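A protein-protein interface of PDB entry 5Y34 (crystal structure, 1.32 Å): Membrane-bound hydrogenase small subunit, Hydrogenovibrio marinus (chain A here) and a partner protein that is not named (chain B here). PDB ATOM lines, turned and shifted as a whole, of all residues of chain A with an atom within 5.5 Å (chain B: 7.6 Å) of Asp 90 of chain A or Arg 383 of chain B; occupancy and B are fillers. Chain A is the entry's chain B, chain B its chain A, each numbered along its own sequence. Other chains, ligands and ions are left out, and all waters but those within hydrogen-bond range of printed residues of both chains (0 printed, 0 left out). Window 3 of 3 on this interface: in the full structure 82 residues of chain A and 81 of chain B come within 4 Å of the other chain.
The guanidinium group of Arg 383 of chain B lies within salt-bridge range of the side-chain carboxylate of Asp 90 of chain A.
N of Ile 386 of chain B lies within hydrogen-bond range of O of Gly 98 of chain A, at 2.8 Å.
Of the 9 printed residues of chain A, 5 touch a printed residue of chain B.
Along chain A the printed residues that touch a printed residue of chain B span positions 89 to 100.
Of the 13 printed residues of chain B, 5 touch a printed residue of chain A.
Along chain B the printed residues that touch a printed residue of chain A span positions 373 to 386.
Among the printed residues, Asp or Glu carboxylates within 4 Å of a Lys or Arg side-chain nitrogen of the other chain: Asp 90 of chain A with Arg 383 of chain B (2.7 Å).
CD2 of Tyr 373 of chain B touches O of Gln 89 of chain A, at 3.9 Å.
Asp 90 of chain A touches Thr 384 of chain B (O to CG2, 3.6 Å).
CE of Met 92 of chain A touches OH of Tyr 373 of chain B (3.3 Å).
CE of Met 92 of chain A touches O of Arg 383 of chain B, 3.4 Å away.
Thr 384 of chain B touches Met 92 of chain A (CA to SD, 3.9 Å).
Ile 386 of chain B touches Met 92 of chain A.
Gly 98 of chain A touches Thr 384 of chain B.
CA of Asn 385 of chain B touches O of Gly 98 of chain A, at 3.3 Å.
Thr 384 of chain B touches Pro 100 of chain A (O to CD, 3.3 Å).
Asn 88 of chain A touches none of the printed residues of chain B.
Of chain B, only Arg 383 and Thr 384 come within 4 Å of Asp 90 of chain A.
Printed residues of chain B within 4 Å of Gly 98 of chain A: Thr 384 (3.5 Å), Asn 385 (3.3 Å) and Ile 386 (2.8 Å).
Gly 381 of chain B touches none of the printed residues of chain A.
Arg 383 of chain B touches two residues of chain A.
Printed residues of chain A within 4 Å of Asn 385 of chain B: Gly 98 (3.3 Å).
The nearest residue of chain B that does not touch Asp 90 of chain A is Tyr 373 of chain B (5.5 Å).
The backbone carbonyl oxygen (O) of Arg 383 of chain B sits at hydrogen-bond distance from the side-chain hydroxyl (OH) of Tyr 373 of chain B (2.7 Å).
The side-chain hydroxyl (OG) of Ser 382 of chain B sits close to the backbone NH (N) of Asn 385 of chain B, at 3.4 Å.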
ATOM      1  N   PRO A  86      28.559   2.236  24.523  1.00  0.00           N
ATOM      2  CA  PRO A  86      27.682   2.795  23.484  1.00  0.00           C
ATOM      3  C   PRO A  86      26.304   2.134  23.498  1.00  0.00           C
ATOM      4  O   PRO A  86      26.179   0.936  23.753  1.00  0.00           O
ATOM      5  CB  PRO A  86      28.414   2.437  22.190  1.00  0.00           C
ATOM      6  CG  PRO A  86      29.121   1.150  22.518  1.00  0.00           C
ATOM      7  CD  PRO A  86      29.477   1.208  23.986  1.00  0.00           C
ATOM      8  N   LEU A  87      25.271   2.926  23.202  1.00  0.00           N
ATOM      9  CA  LEU A  87      23.884   2.445  23.132  1.00  0.00           C
ATOM     10  C   LEU A  87      23.391   2.285  21.692  1.00  0.00           C
ATOM     11  O   LEU A  87      22.425   1.560  21.447  1.00  0.00           O
ATOM     12  CB  LEU A  87      22.915   3.396  23.875  1.00  0.00           C
ATOM     13  CG  LEU A  87      23.214   3.548  25.370  1.00  0.00           C
ATOM     14  CD1 LEU A  87      22.172   4.441  26.024  1.00  0.00           C
ATOM     15  CD2 LEU A  87      23.316   2.213  26.096  1.00  0.00           C
ATOM     16  N   ASN A  88      24.048   2.947  20.741  1.00  0.00           N
ATOM     17  CA  ASN A  88      23.672   2.769  19.338  1.00  0.00           C
ATOM     18  C   ASN A  88      24.307   1.482  18.800  1.00  0.00           C
ATOM     19  O   ASN A  88      25.099   0.846  19.493  1.00  0.00           O
ATOM     20  CB  ASN A  88      24.078   3.966  18.486  1.00  0.00           C
ATOM     21  CG  ASN A  88      23.152   5.154  18.655  1.00  0.00           C
ATOM     22  OD1 ASN A  88      22.069   5.062  19.255  1.00  0.00           O
ATOM     23  ND2 ASN A  88      23.583   6.291  18.121  1.00  0.00           N
ATOM     24  N   GLN A  89      23.947   1.106  17.575  1.00  0.00           N
ATOM     25  CA  GLN A  89      24.416  -0.142  16.957  1.00  0.00           C
ATOM     26  C   GLN A  89      24.087  -1.350  17.837  1.00  0.00           C
ATOM     27  O   GLN A  89      24.802  -2.356  17.814  1.00  0.00           O
ATOM     28  CB  GLN A  89      25.917  -0.066  16.622  1.00  0.00           C
ATOM     29  CG  GLN A  89      26.267   1.054  15.641  1.00  0.00           C
ATOM     30  CD  GLN A  89      26.439   2.422  16.297  1.00  0.00           C
ATOM     31  OE1 GLN A  89      26.942   2.532  17.424  1.00  0.00           O
ATOM     32  NE2 GLN A  89      26.024   3.488  15.584  1.00  0.00           N
ATOM     33  N   ASP A  90      23.004  -1.251  18.609  1.00  0.00           N
ATOM     34  CA  ASP A  90      22.603  -2.278  19.570  1.00  0.00           C
ATOM     35  C   ASP A  90      23.735  -2.604  20.542  1.00  0.00           C
ATOM     36  O   ASP A  90      23.817  -3.710  21.075  1.00  0.00           O
ATOM     37  CB  ASP A  90      22.076  -3.522  18.841  1.00  0.00           C
ATOM     38  CG  ASP A  90      20.676  -3.305  18.279  1.00  0.00           C
ATOM     39  OD1 ASP A  90      19.839  -2.706  18.987  1.00  0.00           O
ATOM     40  OD2 ASP A  90      20.406  -3.719  17.134  1.00  0.00           O
ATOM     41  N   GLY A  91      24.600  -1.621  20.772  1.00  0.00           N
ATOM     42  CA  GLY A  91      25.728  -1.772  21.681  1.00  0.00           C
ATOM     43  C   GLY A  91      26.955  -2.395  21.032  1.00  0.00           C
ATOM     44  O   GLY A  91      28.004  -2.499  21.675  1.00  0.00           O
ATOM     45  N   MET A  92      26.834  -2.763  19.758  1.00  0.00           N
ATOM     46  CA  MET A  92      27.857  -3.575  19.095  1.00  0.00           C
ATOM     47  C   MET A  92      28.912  -2.721  18.389  1.00  0.00           C
ATOM     48  O   MET A  92      29.741  -3.229  17.621  1.00  0.00           O
ATOM     49  CB  MET A  92      27.220  -4.602  18.163  1.00  0.00           C
ATOM     50  CG  MET A  92      26.266  -5.556  18.881  1.00  0.00           C
ATOM     51  SD  MET A  92      27.114  -6.635  20.079  1.00  0.00           S
ATOM     52  CE  MET A  92      27.813  -7.916  19.040  1.00  0.00           C
ATOM     53  N   GLY A  98      31.881 -11.300  21.989  1.00  0.00           N
ATOM     54  CA  GLY A  98      30.749 -11.410  21.068  1.00  0.00           C
ATOM     55  C   GLY A  98      29.471 -10.688  21.477  1.00  0.00           C
ATOM     56  O   GLY A  98      28.468 -10.774  20.766  1.00  0.00           O
ATOM     57  N   PRO A 100      27.524  -7.050  23.579  1.00  0.00           N
ATOM     58  CA  PRO A 100      27.800  -5.641  23.842  1.00  0.00           C
ATOM     59  C   PRO A 100      28.569  -5.433  25.145  1.00  0.00           C
ATOM     60  O   PRO A 100      28.276  -6.089  26.149  1.00  0.00           O
ATOM     61  CB  PRO A 100      26.405  -5.015  23.968  1.00  0.00           C
ATOM     62  CG  PRO A 100      25.482  -5.961  23.295  1.00  0.00           C
ATOM     63  CD  PRO A 100      26.081  -7.331  23.459  1.00  0.00           C
ATOM     64  N   TRP B 352      31.944  -2.818   8.637  1.00  0.00           N
ATOM     65  CA  TRP B 352      30.647  -2.285   9.093  1.00  0.00           C
ATOM     66  C   TRP B 352      30.403  -0.810   8.767  1.00  0.00           C
ATOM     67  O   TRP B 352      30.130  -0.005   9.655  1.00  0.00           O
ATOM     68  CB  TRP B 352      30.435  -2.578  10.581  1.00  0.00           C
ATOM     69  CG  TRP B 352      30.268  -4.067  10.828  1.00  0.00           C
ATOM     70  CD1 TRP B 352      29.475  -4.934  10.117  1.00  0.00           C
ATOM     71  CD2 TRP B 352      30.915  -4.861  11.838  1.00  0.00           C
ATOM     72  NE1 TRP B 352      29.581  -6.218  10.630  1.00  0.00           N
ATOM     73  CE2 TRP B 352      30.449  -6.196  11.693  1.00  0.00           C
ATOM     74  CE3 TRP B 352      31.779  -4.551  12.883  1.00  0.00           C
ATOM     75  CZ2 TRP B 352      30.876  -7.241  12.528  1.00  0.00           C
ATOM     76  CZ3 TRP B 352      32.238  -5.608  13.712  1.00  0.00           C
ATOM     77  CH2 TRP B 352      31.768  -6.938  13.525  1.00  0.00           C
ATOM     78  N   ASN B 372      27.452   0.843   9.485  1.00  0.00           N
ATOM     79  CA  ASN B 372      26.514  -0.161   9.004  1.00  0.00           C
ATOM     80  C   ASN B 372      26.836  -1.493   9.692  1.00  0.00           C
ATOM     81  O   ASN B 372      27.446  -2.401   9.088  1.00  0.00           O
ATOM     82  CB  ASN B 372      26.593  -0.271   7.470  1.00  0.00           C
ATOM     83  CG  ASN B 372      25.618  -1.284   6.895  1.00  0.00           C
ATOM     84  OD1 ASN B 372      25.987  -2.142   6.084  1.00  0.00           O
ATOM     85  ND2 ASN B 372      24.372  -1.197   7.321  1.00  0.00           N
ATOM     86  N   TYR B 373      26.461  -1.596  10.969  1.00  0.00           N
ATOM     87  CA  TYR B 373      26.679  -2.832  11.716  1.00  0.00           C
ATOM     88  C   TYR B 373      25.628  -3.850  11.253  1.00  0.00           C
ATOM     89  O   TYR B 373      24.433  -3.694  11.505  1.00  0.00           O
ATOM     90  CB  TYR B 373      26.635  -2.600  13.236  1.00  0.00           C
ATOM     91  CG  TYR B 373      26.719  -3.903  13.979  1.00  0.00           C
ATOM     92  CD1 TYR B 373      27.910  -4.649  13.987  1.00  0.00           C
ATOM     93  CD2 TYR B 373      25.603  -4.433  14.609  1.00  0.00           C
ATOM     94  CE1 TYR B 373      27.967  -5.876  14.625  1.00  0.00           C
ATOM     95  CE2 TYR B 373      25.653  -5.663  15.248  1.00  0.00           C
ATOM     96  CZ  TYR B 373      26.837  -6.379  15.250  1.00  0.00           C
ATOM     97  OH  TYR B 373      26.905  -7.590  15.894  1.00  0.00           O
ATOM     98  N   GLU B 374      26.100  -4.899  10.574  1.00  0.00           N
ATOM     99  CA  GLU B 374      25.219  -5.845   9.914  1.00  0.00           C
ATOM    100  C   GLU B 374      26.011  -7.139   9.815  1.00  0.00           C
ATOM    101  O   GLU B 374      27.133  -7.151   9.280  1.00  0.00           O
ATOM    102  CB  GLU B 374      24.874  -5.377   8.508  1.00  0.00           C
ATOM    103  CG  GLU B 374      23.988  -6.322   7.715  1.00  0.00           C
ATOM    104  CD  GLU B 374      23.518  -5.695   6.422  1.00  0.00           C
ATOM    105  OE1 GLU B 374      24.371  -5.352   5.586  1.00  0.00           O
ATOM    106  OE2 GLU B 374      22.298  -5.530   6.251  1.00  0.00           O
ATOM    107  N   LEU B 375      25.428  -8.215  10.331  1.00  0.00           N
ATOM    108  CA  LEU B 375      26.103  -9.517  10.317  1.00  0.00           C
ATOM    109  C   LEU B 375      25.654 -10.345   9.130  1.00  0.00           C
ATOM    110  O   LEU B 375      24.478 -10.315   8.743  1.00  0.00           O
ATOM    111  CB  LEU B 375      25.812 -10.263  11.619  1.00  0.00           C
ATOM    112  CG  LEU B 375      26.285  -9.619  12.928  1.00  0.00           C
ATOM    113  CD1 LEU B 375      26.100 -10.588  14.089  1.00  0.00           C
ATOM    114  CD2 LEU B 375      27.723  -9.134  12.835  1.00  0.00           C
ATOM    115  N   THR B 379      26.312 -16.148   9.926  1.00  0.00           N
ATOM    116  CA  THR B 379      26.761 -15.962  11.308  1.00  0.00           C
ATOM    117  C   THR B 379      26.179 -17.053  12.215  1.00  0.00           C
ATOM    118  O   THR B 379      25.005 -17.399  12.102  1.00  0.00           O
ATOM    119  CB  THR B 379      26.310 -14.577  11.838  1.00  0.00           C
ATOM    120  OG1 THR B 379      26.867 -13.551  11.014  1.00  0.00           O
ATOM    121  CG2 THR B 379      26.756 -14.351  13.284  1.00  0.00           C
ATOM    122  N   LYS B 380      27.027 -17.624  13.073  1.00  0.00           N
ATOM    123  CA  LYS B 380      26.540 -18.444  14.175  1.00  0.00           C
ATOM    124  C   LYS B 380      26.336 -17.508  15.363  1.00  0.00           C
ATOM    125  O   LYS B 380      27.267 -16.819  15.790  1.00  0.00           O
ATOM    126  CB  LYS B 380      27.517 -19.578  14.512  1.00  0.00           C
ATOM    127  CG  LYS B 380      27.005 -20.533  15.582  1.00  0.00           C
ATOM    128  CD  LYS B 380      27.996 -21.651  15.876  1.00  0.00           C
ATOM    129  CE  LYS B 380      27.983 -22.710  14.785  1.00  0.00           C
ATOM    130  NZ  LYS B 380      28.516 -22.194  13.495  1.00  0.00           N
ATOM    131  N   GLY B 381      25.106 -17.466  15.866  1.00  0.00           N
ATOM    132  CA  GLY B 381      24.731 -16.554  16.939  1.00  0.00           C
ATOM    133  C   GLY B 381      23.705 -15.530  16.492  1.00  0.00           C
ATOM    134  O   GLY B 381      22.958 -15.762  15.540  1.00  0.00           O
ATOM    135  N   SER B 382      23.670 -14.396  17.179  1.00  0.00           N
ATOM    136  CA  SER B 382      22.702 -13.344  16.885  1.00  0.00           C
ATOM    137  C   SER B 382      23.388 -11.982  16.819  1.00  0.00           C
ATOM    138  O   SER B 382      24.604 -11.881  17.029  1.00  0.00           O
ATOM    139  CB  SER B 382      21.595 -13.344  17.941  1.00  0.00           C
ATOM    140  OG  SER B 382      22.127 -13.072  19.232  1.00  0.00           O
ATOM    141  N   ARG B 383      22.604 -10.945  16.531  1.00  0.00           N
ATOM    142  CA  ARG B 383      23.136  -9.592  16.370  1.00  0.00           C
ATOM    143  C   ARG B 383      23.896  -9.093  17.598  1.00  0.00           C
ATOM    144  O   ARG B 383      24.856  -8.336  17.466  1.00  0.00           O
ATOM    145  CB  ARG B 383      22.014  -8.614  16.010  1.00  0.00           C
ATOM    146  CG  ARG B 383      22.483  -7.193  15.695  1.00  0.00           C
ATOM    147  CD  ARG B 383      21.342  -6.351  15.140  1.00  0.00           C
ATOM    148  NE  ARG B 383      21.630  -4.906  15.033  1.00  0.00           N
ATOM    149  CZ  ARG B 383      22.208  -4.340  13.982  1.00  0.00           C
ATOM    150  NH1 ARG B 383      22.631  -5.107  12.968  1.00  0.00           N
ATOM    151  NH2 ARG B 383      22.396  -3.018  13.954  1.00  0.00           N
ATOM    152  N   THR B 384      23.462  -9.506  18.786  1.00  0.00           N
ATOM    153  CA  THR B 384      24.128  -9.078  20.017  1.00  0.00           C
ATOM    154  C   THR B 384      24.813 -10.243  20.719  1.00  0.00           C
ATOM    155  O   THR B 384      25.178 -10.143  21.891  1.00  0.00           O
ATOM    156  CB  THR B 384      23.173  -8.356  20.992  1.00  0.00           C
ATOM    157  OG1 THR B 384      22.101  -9.234  21.351  1.00  0.00           O
ATOM    158  CG2 THR B 384      22.612  -7.072  20.366  1.00  0.00           C
ATOM    159  N   ASN B 385      25.003 -11.339  19.988  1.00  0.00           N
ATOM    160  CA  ASN B 385      25.706 -12.493  20.526  1.00  0.00           C
ATOM    161  C   ASN B 385      26.394 -13.271  19.414  1.00  0.00           C
ATOM    162  O   ASN B 385      25.854 -14.260  18.910  1.00  0.00           O
ATOM    163  CB  ASN B 385      24.762 -13.408  21.321  1.00  0.00           C
ATOM    164  CG  ASN B 385      25.477 -14.626  21.886  1.00  0.00           C
ATOM    165  OD1 ASN B 385      26.655 -14.557  22.261  1.00  0.00           O
ATOM    166  ND2 ASN B 385      24.777 -15.755  21.928  1.00  0.00           N
ATOM    167  N   ILE B 386      27.595 -12.830  19.048  1.00  0.00           N
ATOM    168  CA  ILE B 386      28.327 -13.453  17.951  1.00  0.00           C
ATOM    169  C   ILE B 386      29.073 -14.677  18.487  1.00  0.00           C
ATOM    170  O   ILE B 386      29.948 -14.549  19.349  1.00  0.00           O
ATOM    171  CB  ILE B 386      29.326 -12.472  17.294  1.00  0.00           C
ATOM    172  CG1 ILE B 386      28.623 -11.161  16.907  1.00  0.00           C
ATOM    173  CG2 ILE B 386      30.008 -13.125  16.095  1.00  0.00           C
ATOM    174  CD1 ILE B 386      29.567 -10.106  16.371  1.00  0.00           C
